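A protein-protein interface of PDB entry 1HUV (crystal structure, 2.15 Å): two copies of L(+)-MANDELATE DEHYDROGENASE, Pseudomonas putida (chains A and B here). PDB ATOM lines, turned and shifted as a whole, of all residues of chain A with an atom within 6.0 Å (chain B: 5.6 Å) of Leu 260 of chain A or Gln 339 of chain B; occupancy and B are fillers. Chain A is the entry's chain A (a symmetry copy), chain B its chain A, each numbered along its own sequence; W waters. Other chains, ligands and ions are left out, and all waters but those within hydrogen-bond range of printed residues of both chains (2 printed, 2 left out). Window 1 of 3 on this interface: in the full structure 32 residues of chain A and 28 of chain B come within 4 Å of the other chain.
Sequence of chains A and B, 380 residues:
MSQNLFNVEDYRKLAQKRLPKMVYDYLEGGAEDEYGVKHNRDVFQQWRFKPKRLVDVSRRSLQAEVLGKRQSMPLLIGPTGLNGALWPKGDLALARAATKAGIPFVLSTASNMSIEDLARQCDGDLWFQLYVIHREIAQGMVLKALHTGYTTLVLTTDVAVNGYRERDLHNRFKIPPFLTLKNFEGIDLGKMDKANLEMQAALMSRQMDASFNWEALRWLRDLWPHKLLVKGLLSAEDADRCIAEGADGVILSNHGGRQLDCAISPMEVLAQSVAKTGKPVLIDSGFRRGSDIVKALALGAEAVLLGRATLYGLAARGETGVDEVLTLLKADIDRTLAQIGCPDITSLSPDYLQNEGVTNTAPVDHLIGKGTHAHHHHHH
No position is printed for both chains.
Hydrophobic or aromatic side chains of chain A that line the printed part of chain B: Val 161, Tyr 164 and Leu 260. Along chain A the printed residues that touch a printed residue of chain B span positions 158 to 263. Hydrophobic or aromatic side chains of chain B that line the printed part of chain A: Phe 49, Ala 338 and Ile 340. Among the printed residues, 12 pairs touch across the chains.
The backbone carbonyl oxygen (O) of Gln 339 of chain B lies within hydrogen-bond range of the guanidinium group (NH1) of Arg 53 of chain B (2.7 Å). N of Lys 52 of chain B is in hydrogen-bond range of O of Ile 340 of chain B (2.9 Å). O of Asp 158 of chain A sits at hydrogen-bond distance from NE2 of Gln 259 of chain A (3.1 Å). The side-chain amide oxygen of Gln 259 of chain A is in hydrogen-bond range of the backbone NH of Gly 163 of chain A (3.2 Å). The backbone carbonyl oxygen (O) of Arg 335 of chain B is in hydrogen-bond range of the side-chain amide nitrogen (NE2) of Gln 339 of chain B (3.1 Å). NE2 of Gln 259 of chain A lies within hydrogen-bond range of O of Val 161 of chain A (2.9 Å).
Of the printed residues of chain B, Val 161 of chain A touches Ala 338 (3.9 Å). Arg 258 of chain A touches none of the printed residues of chain B. Leu 260 of chain A touches just these residues of chain B: Phe 49 (3.6 Å), Gln 339 (3.9 Å) and Ile 340 (3.8 Å). Printed residues of chain A within 4 Å of Gln 339 of chain B: Asn 162, Gly 163, Gln 259 and Leu 260. Of the printed residues of chain A, Ile 340 of chain B touches Leu 260 (3.8 Å). The nearest residue of chain B that does not touch Leu 260 of chain A is Pro 51 of chain B (4.4 Å).
OE1 of Gln 339 of chain B sits close to O of Gln 259 of chain A, at 2.8 Å. O of Cys 262 of chain A lies within hydrogen-bond range of N of Phe 49 of chain B (2.8 Å).
Asp 158 of chain A touches Arg 53 of chain B. Val 161 of chain A touches Ala 338 of chain B (CG2 to CB, 3.9 Å). O of Asn 162 of chain A touches CD of Arg 335 of chain B, 3.8 Å away. OE1 of Gln 339 of chain B touches O of Asn 162 of chain A (3.98 Å). Gln 339 of chain B touches Gly 163 of chain A (OE1 to CA, 3.99 Å). Tyr 164 of chain A touches Arg 335 of chain B (CD1 to CZ, 3.2 Å). CD2 of Phe 49 of chain B touches CD1 of Leu 260 of chain A, 3.6 Å away. Leu 260 of chain A touches Gln 339 of chain B (CG to CB, 3.9 Å). Leu 260 of chain A touches Ile 340 of chain B (CD1 to CG2, 3.8 Å). Phe 49 of chain B touches Ala 263 of chain A.
Water W2 lies within hydrogen-bond range of the backbone carbonyl oxygen (O) of Gln 259 of chain A (2.6 Å), the backbone NH (N) of Tyr 164 of chain A (2.9 Å) and the side-chain amide oxygen (OE1) of Gln 339 of chain B (3.0 Å). Water W1 lies within hydrogen-bond range of the guanidinium group of Arg 53 of chain B and the side-chain carboxylate of Asp 158 of chain A.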
ATOM      1  N   ALA A  31      26.901 -36.443   6.161  1.00  0.00           N
ATOM      2  CA  ALA A  31      25.647 -36.000   5.566  1.00  0.00           C
ATOM      3  C   ALA A  31      25.314 -36.778   4.293  1.00  0.00           C
ATOM      4  O   ALA A  31      26.200 -37.133   3.517  1.00  0.00           O
ATOM      5  CB  ALA A  31      25.724 -34.509   5.252  1.00  0.00           C
ATOM      6  N   GLY A  36      30.905 -36.598   0.814  1.00  0.00           N
ATOM      7  CA  GLY A  36      31.711 -35.564   1.433  1.00  0.00           C
ATOM      8  C   GLY A  36      32.868 -36.115   2.249  1.00  0.00           C
ATOM      9  O   GLY A  36      34.019 -35.743   2.011  1.00  0.00           O
ATOM     10  N   ASP A 158      29.064 -23.097  10.738  1.00  0.00           N
ATOM     11  CA  ASP A 158      28.489 -23.988   9.737  1.00  0.00           C
ATOM     12  C   ASP A 158      27.368 -24.913  10.183  1.00  0.00           C
ATOM     13  O   ASP A 158      27.204 -25.999   9.629  1.00  0.00           O
ATOM     14  CB  ASP A 158      29.590 -24.811   9.049  1.00  0.00           C
ATOM     15  CG  ASP A 158      30.427 -25.604  10.019  1.00  0.00           C
ATOM     16  OD1 ASP A 158      30.073 -25.672  11.211  1.00  0.00           O
ATOM     17  OD2 ASP A 158      31.456 -26.184   9.584  1.00  0.00           O
ATOM     18  N   ALA A 160      24.023 -23.481  10.830  1.00  0.00           N
ATOM     19  CA  ALA A 160      22.876 -22.572  10.843  1.00  0.00           C
ATOM     20  C   ALA A 160      21.637 -23.441  10.973  1.00  0.00           C
ATOM     21  O   ALA A 160      20.627 -23.049  11.554  1.00  0.00           O
ATOM     22  CB  ALA A 160      22.821 -21.773   9.548  1.00  0.00           C
ATOM     23  N   VAL A 161      21.750 -24.636  10.404  1.00  0.00           N
ATOM     24  CA  VAL A 161      20.702 -25.644  10.422  1.00  0.00           C
ATOM     25  C   VAL A 161      21.428 -26.978  10.568  1.00  0.00           C
ATOM     26  O   VAL A 161      22.621 -27.078  10.271  1.00  0.00           O
ATOM     27  CB  VAL A 161      19.874 -25.616   9.121  1.00  0.00           C
ATOM     28  CG1 VAL A 161      19.106 -26.892   8.974  1.00  0.00           C
ATOM     29  CG2 VAL A 161      18.915 -24.437   9.132  1.00  0.00           C
ATOM     30  N   ASN A 162      20.719 -27.995  11.043  1.00  0.00           N
ATOM     31  CA  ASN A 162      21.324 -29.311  11.249  1.00  0.00           C
ATOM     32  C   ASN A 162      21.557 -30.094   9.961  1.00  0.00           C
ATOM     33  O   ASN A 162      20.758 -30.042   9.024  1.00  0.00           O
ATOM     34  CB  ASN A 162      20.446 -30.131  12.188  1.00  0.00           C
ATOM     35  CG  ASN A 162      20.217 -29.437  13.521  1.00  0.00           C
ATOM     36  OD1 ASN A 162      19.233 -29.705  14.216  1.00  0.00           O
ATOM     37  ND2 ASN A 162      21.135 -28.542  13.888  1.00  0.00           N
ATOM     38  N   GLY A 163      22.664 -30.827   9.927  1.00  0.00           N
ATOM     39  CA  GLY A 163      22.989 -31.632   8.762  1.00  0.00           C
ATOM     40  C   GLY A 163      22.071 -32.832   8.641  1.00  0.00           C
ATOM     41  O   GLY A 163      21.658 -33.410   9.647  1.00  0.00           O
ATOM     42  N   TYR A 164      21.747 -33.208   7.409  1.00  0.00           N
ATOM     43  CA  TYR A 164      20.875 -34.353   7.175  1.00  0.00           C
ATOM     44  C   TYR A 164      21.705 -35.637   7.176  1.00  0.00           C
ATOM     45  O   TYR A 164      22.125 -36.113   6.123  1.00  0.00           O
ATOM     46  CB  TYR A 164      20.152 -34.190   5.834  1.00  0.00           C
ATOM     47  CG  TYR A 164      18.869 -34.987   5.704  1.00  0.00           C
ATOM     48  CD1 TYR A 164      17.733 -34.634   6.426  1.00  0.00           C
ATOM     49  CD2 TYR A 164      18.783 -36.074   4.838  1.00  0.00           C
ATOM     50  CE1 TYR A 164      16.539 -35.337   6.286  1.00  0.00           C
ATOM     51  CE2 TYR A 164      17.590 -36.788   4.691  1.00  0.00           C
ATOM     52  CZ  TYR A 164      16.471 -36.413   5.417  1.00  0.00           C
ATOM     53  OH  TYR A 164      15.284 -37.104   5.273  1.00  0.00           O
ATOM     54  N   ASN A 254      34.694 -28.090   6.807  1.00  0.00           N
ATOM     55  CA  ASN A 254      33.366 -28.462   6.336  1.00  0.00           C
ATOM     56  C   ASN A 254      32.728 -29.358   7.402  1.00  0.00           C
ATOM     57  O   ASN A 254      31.857 -30.183   7.135  1.00  0.00           O
ATOM     58  CB  ASN A 254      33.356 -29.114   4.922  1.00  0.00           C
ATOM     59  CG  ASN A 254      34.128 -30.425   4.828  1.00  0.00           C
ATOM     60  OD1 ASN A 254      34.215 -31.200   5.778  1.00  0.00           O
ATOM     61  ND2 ASN A 254      34.664 -30.689   3.632  1.00  0.00           N
ATOM     62  N   GLY A 257      32.595 -33.295   6.983  1.00  0.00           N
ATOM     63  CA  GLY A 257      31.587 -33.881   6.116  1.00  0.00           C
ATOM     64  C   GLY A 257      30.211 -34.149   6.708  1.00  0.00           C
ATOM     65  O   GLY A 257      29.395 -34.815   6.069  1.00  0.00           O
ATOM     66  N   ARG A 258      29.932 -33.622   7.898  1.00  0.00           N
ATOM     67  CA  ARG A 258      28.644 -33.863   8.526  1.00  0.00           C
ATOM     68  C   ARG A 258      27.553 -32.834   8.271  1.00  0.00           C
ATOM     69  O   ARG A 258      26.428 -33.013   8.732  1.00  0.00           O
ATOM     70  CB  ARG A 258      28.813 -33.981  10.025  1.00  0.00           C
ATOM     71  CG  ARG A 258      30.126 -34.532  10.466  1.00  0.00           C
ATOM     72  CD  ARG A 258      30.032 -34.651  11.948  1.00  0.00           C
ATOM     73  NE  ARG A 258      30.204 -35.993  12.457  1.00  0.00           N
ATOM     74  CZ  ARG A 258      29.331 -36.614  13.240  1.00  0.00           C
ATOM     75  NH1 ARG A 258      28.219 -36.017  13.607  1.00  0.00           N
ATOM     76  NH2 ARG A 258      29.607 -37.827  13.699  1.00  0.00           N
ATOM     77  N   GLN A 259      27.858 -31.769   7.545  1.00  0.00           N
ATOM     78  CA  GLN A 259      26.844 -30.752   7.312  1.00  0.00           C
ATOM     79  C   GLN A 259      26.274 -30.645   5.917  1.00  0.00           C
ATOM     80  O   GLN A 259      25.050 -30.595   5.739  1.00  0.00           O
ATOM     81  CB  GLN A 259      27.375 -29.384   7.739  1.00  0.00           C
ATOM     82  CG  GLN A 259      27.435 -29.190   9.248  1.00  0.00           C
ATOM     83  CD  GLN A 259      26.073 -29.348   9.889  1.00  0.00           C
ATOM     84  OE1 GLN A 259      25.802 -30.344  10.561  1.00  0.00           O
ATOM     85  NE2 GLN A 259      25.203 -28.372   9.670  1.00  0.00           N
ATOM     86  N   LEU A 260      27.161 -30.596   4.926  1.00  0.00           N
ATOM     87  CA  LEU A 260      26.756 -30.460   3.529  1.00  0.00           C
ATOM     88  C   LEU A 260      27.551 -31.491   2.744  1.00  0.00           C
ATOM     89  O   LEU A 260      28.751 -31.321   2.543  1.00  0.00           O
ATOM     90  CB  LEU A 260      27.120 -29.052   3.035  1.00  0.00           C
ATOM     91  CG  LEU A 260      26.249 -28.266   2.062  1.00  0.00           C
ATOM     92  CD1 LEU A 260      27.144 -27.301   1.307  1.00  0.00           C
ATOM     93  CD2 LEU A 260      25.533 -29.185   1.114  1.00  0.00           C
ATOM     94  N   ASP A 261      26.891 -32.544   2.277  1.00  0.00           N
ATOM     95  CA  ASP A 261      27.606 -33.594   1.553  1.00  0.00           C
ATOM     96  C   ASP A 261      28.440 -33.136   0.358  1.00  0.00           C
ATOM     97  O   ASP A 261      29.513 -33.691   0.129  1.00  0.00           O
ATOM     98  CB  ASP A 261      26.642 -34.714   1.125  1.00  0.00           C
ATOM     99  CG  ASP A 261      27.357 -36.031   0.891  1.00  0.00           C
ATOM    100  OD1 ASP A 261      28.335 -36.326   1.617  1.00  0.00           O
ATOM    101  OD2 ASP A 261      26.944 -36.793  -0.005  1.00  0.00           O
ATOM    102  N   CYS A 262      27.982 -32.123  -0.377  1.00  0.00           N
ATOM    103  CA  CYS A 262      28.733 -31.664  -1.541  1.00  0.00           C
ATOM    104  C   CYS A 262      29.638 -30.453  -1.317  1.00  0.00           C
ATOM    105  O   CYS A 262      30.096 -29.829  -2.277  1.00  0.00           O
ATOM    106  CB  CYS A 262      27.776 -31.397  -2.701  1.00  0.00           C
ATOM    107  SG  CYS A 262      26.852 -32.860  -3.207  1.00  0.00           S
ATOM    108  N   ALA A 263      29.926 -30.137  -0.059  1.00  0.00           N
ATOM    109  CA  ALA A 263      30.810 -29.017   0.240  1.00  0.00           C
ATOM    110  C   ALA A 263      32.214 -29.366  -0.250  1.00  0.00           C
ATOM    111  O   ALA A 263      32.598 -30.539  -0.264  1.00  0.00           O
ATOM    112  CB  ALA A 263      30.831 -28.759   1.746  1.00  0.00           C
ATOM    113  N   PHE B  49      30.048 -27.311  -3.511  1.00  0.00           N
ATOM    114  CA  PHE B  49      29.624 -26.049  -2.924  1.00  0.00           C
ATOM    115  C   PHE B  49      30.679 -25.271  -2.157  1.00  0.00           C
ATOM    116  O   PHE B  49      31.517 -25.840  -1.455  1.00  0.00           O
ATOM    117  CB  PHE B  49      28.440 -26.277  -1.976  1.00  0.00           C
ATOM    118  CG  PHE B  49      27.187 -26.748  -2.659  1.00  0.00           C
ATOM    119  CD1 PHE B  49      26.655 -26.040  -3.729  1.00  0.00           C
ATOM    120  CD2 PHE B  49      26.520 -27.881  -2.205  1.00  0.00           C
ATOM    121  CE1 PHE B  49      25.472 -26.452  -4.341  1.00  0.00           C
ATOM    122  CE2 PHE B  49      25.335 -28.303  -2.806  1.00  0.00           C
ATOM    123  CZ  PHE B  49      24.810 -27.584  -3.878  1.00  0.00           C
ATOM    124  N   PRO B  51      29.980 -22.576   0.274  1.00  0.00           N
ATOM    125  CA  PRO B  51      28.999 -21.752   0.977  1.00  0.00           C
ATOM    126  C   PRO B  51      29.516 -20.406   1.447  1.00  0.00           C
ATOM    127  O   PRO B  51      30.723 -20.206   1.620  1.00  0.00           O
ATOM    128  CB  PRO B  51      28.538 -22.645   2.137  1.00  0.00           C
ATOM    129  CG  PRO B  51      29.582 -23.711   2.244  1.00  0.00           C
ATOM    130  CD  PRO B  51      30.046 -23.935   0.840  1.00  0.00           C
ATOM    131  N   LYS B  52      28.580 -19.480   1.626  1.00  0.00           N
ATOM    132  CA  LYS B  52      28.884 -18.140   2.100  1.00  0.00           C
ATOM    133  C   LYS B  52      28.441 -18.130   3.560  1.00  0.00           C
ATOM    134  O   LYS B  52      27.255 -18.258   3.857  1.00  0.00           O
ATOM    135  CB  LYS B  52      28.098 -17.106   1.284  1.00  0.00           C
ATOM    136  CG  LYS B  52      28.388 -17.156  -0.219  1.00  0.00           C
ATOM    137  CD  LYS B  52      27.707 -16.016  -0.972  1.00  0.00           C
ATOM    138  CE  LYS B  52      27.987 -16.085  -2.472  1.00  0.00           C
ATOM    139  NZ  LYS B  52      29.444 -16.159  -2.782  1.00  0.00           N
ATOM    140  N   ARG B  53      29.401 -18.005   4.470  1.00  0.00           N
ATOM    141  CA  ARG B  53      29.100 -18.012   5.897  1.00  0.00           C
ATOM    142  C   ARG B  53      28.688 -16.651   6.451  1.00  0.00           C
ATOM    143  O   ARG B  53      28.896 -15.615   5.820  1.00  0.00           O
ATOM    144  CB  ARG B  53      30.301 -18.525   6.694  1.00  0.00           C
ATOM    145  CG  ARG B  53      30.677 -19.975   6.425  1.00  0.00           C
ATOM    146  CD  ARG B  53      29.554 -20.930   6.786  1.00  0.00           C
ATOM    147  NE  ARG B  53      29.921 -22.306   6.470  1.00  0.00           N
ATOM    148  CZ  ARG B  53      29.095 -23.188   5.923  1.00  0.00           C
ATOM    149  NH1 ARG B  53      27.850 -22.837   5.634  1.00  0.00           N
ATOM    150  NH2 ARG B  53      29.517 -24.413   5.648  1.00  0.00           N
ATOM    151  N   ASP B 334      15.521 -26.511   0.685  1.00  0.00           N
ATOM    152  CA  ASP B 334      15.522 -25.478   1.722  1.00  0.00           C
ATOM    153  C   ASP B 334      16.746 -25.569   2.631  1.00  0.00           C
ATOM    154  O   ASP B 334      17.391 -24.563   2.945  1.00  0.00           O
ATOM    155  CB  ASP B 334      14.259 -25.607   2.578  1.00  0.00           C
ATOM    156  CG  ASP B 334      14.298 -24.729   3.808  1.00  0.00           C
ATOM    157  OD1 ASP B 334      14.198 -23.492   3.664  1.00  0.00           O
ATOM    158  OD2 ASP B 334      14.444 -25.277   4.919  1.00  0.00           O
ATOM    159  N   ARG B 335      17.046 -26.785   3.064  1.00  0.00           N
ATOM    160  CA  ARG B 335      18.179 -27.042   3.938  1.00  0.00           C
ATOM    161  C   ARG B 335      19.491 -26.684   3.225  1.00  0.00           C
ATOM    162  O   ARG B 335      20.407 -26.118   3.827  1.00  0.00           O
ATOM    163  CB  ARG B 335      18.157 -28.520   4.339  1.00  0.00           C
ATOM    164  CG  ARG B 335      19.185 -28.943   5.360  1.00  0.00           C
ATOM    165  CD  ARG B 335      19.111 -30.450   5.606  1.00  0.00           C
ATOM    166  NE  ARG B 335      17.814 -30.869   6.136  1.00  0.00           N
ATOM    167  CZ  ARG B 335      16.936 -31.628   5.483  1.00  0.00           C
ATOM    168  NH1 ARG B 335      17.201 -32.066   4.259  1.00  0.00           N
ATOM    169  NH2 ARG B 335      15.788 -31.953   6.061  1.00  0.00           N
ATOM    170  N   THR B 336      19.567 -27.005   1.936  1.00  0.00           N
ATOM    171  CA  THR B 336      20.762 -26.724   1.145  1.00  0.00           C
ATOM    172  C   THR B 336      20.974 -25.224   1.002  1.00  0.00           C
ATOM    173  O   THR B 336      22.103 -24.736   1.073  1.00  0.00           O
ATOM    174  CB  THR B 336      20.661 -27.348  -0.258  1.00  0.00           C
ATOM    175  OG1 THR B 336      20.518 -28.768  -0.133  1.00  0.00           O
ATOM    176  CG2 THR B 336      21.913 -27.040  -1.072  1.00  0.00           C
ATOM    177  N   LEU B 337      19.887 -24.492   0.797  1.00  0.00           N
ATOM    178  CA  LEU B 337      19.995 -23.050   0.671  1.00  0.00           C
ATOM    179  C   LEU B 337      20.564 -22.476   1.971  1.00  0.00           C
ATOM    180  O   LEU B 337      21.465 -21.645   1.941  1.00  0.00           O
ATOM    181  CB  LEU B 337      18.622 -22.439   0.354  1.00  0.00           C
ATOM    182  CG  LEU B 337      18.030 -22.777  -1.021  1.00  0.00           C
ATOM    183  CD1 LEU B 337      16.694 -22.070  -1.186  1.00  0.00           C
ATOM    184  CD2 LEU B 337      18.993 -22.354  -2.130  1.00  0.00           C
ATOM    185  N   ALA B 338      20.059 -22.936   3.111  1.00  0.00           N
ATOM    186  CA  ALA B 338      20.545 -22.445   4.400  1.00  0.00           C
ATOM    187  C   ALA B 338      22.036 -22.718   4.549  1.00  0.00           C
ATOM    188  O   ALA B 338      22.812 -21.836   4.916  1.00  0.00           O
ATOM    189  CB  ALA B 338      19.790 -23.113   5.543  1.00  0.00           C
ATOM    190  N   GLN B 339      22.421 -23.952   4.251  1.00  0.00           N
ATOM    191  CA  GLN B 339      23.802 -24.386   4.367  1.00  0.00           C
ATOM    192  C   GLN B 339      24.801 -23.663   3.476  1.00  0.00           C
ATOM    193  O   GLN B 339      25.958 -23.500   3.862  1.00  0.00           O
ATOM    194  CB  GLN B 339      23.876 -25.892   4.137  1.00  0.00           C
ATOM    195  CG  GLN B 339      23.379 -26.691   5.331  1.00  0.00           C
ATOM    196  CD  GLN B 339      22.909 -28.075   4.951  1.00  0.00           C
ATOM    197  OE1 GLN B 339      22.819 -28.966   5.795  1.00  0.00           O
ATOM    198  NE2 GLN B 339      22.587 -28.260   3.678  1.00  0.00           N
ATOM    199  N   ILE B 340      24.380 -23.229   2.290  1.00  0.00           N
ATOM    200  CA  ILE B 340      25.300 -22.516   1.408  1.00  0.00           C
ATOM    201  C   ILE B 340      25.149 -21.001   1.557  1.00  0.00           C
ATOM    202  O   ILE B 340      25.848 -20.224   0.903  1.00  0.00           O
ATOM    203  CB  ILE B 340      25.117 -22.920  -0.092  1.00  0.00           C
ATOM    204  CG1 ILE B 340      23.764 -22.438  -0.624  1.00  0.00           C
ATOM    205  CG2 ILE B 340      25.258 -24.434  -0.236  1.00  0.00           C
ATOM    206  CD1 ILE B 340      23.606 -22.601  -2.139  1.00  0.00           C
ATOM    207  N   GLY B 341      24.237 -20.583   2.427  1.00  0.00           N
ATOM    208  CA  GLY B 341      24.040 -19.162   2.658  1.00  0.00           C
ATOM    209  C   GLY B 341      23.347 -18.371   1.565  1.00  0.00           C
ATOM    210  O   GLY B 341      23.707 -17.223   1.308  1.00  0.00           O
HETATM  211  O   HOH W   1      31.452 -25.829   6.779  1.00  0.00           O
HETATM  212  O   HOH W   2      22.866 -31.898   5.087  1.00  0.00           O
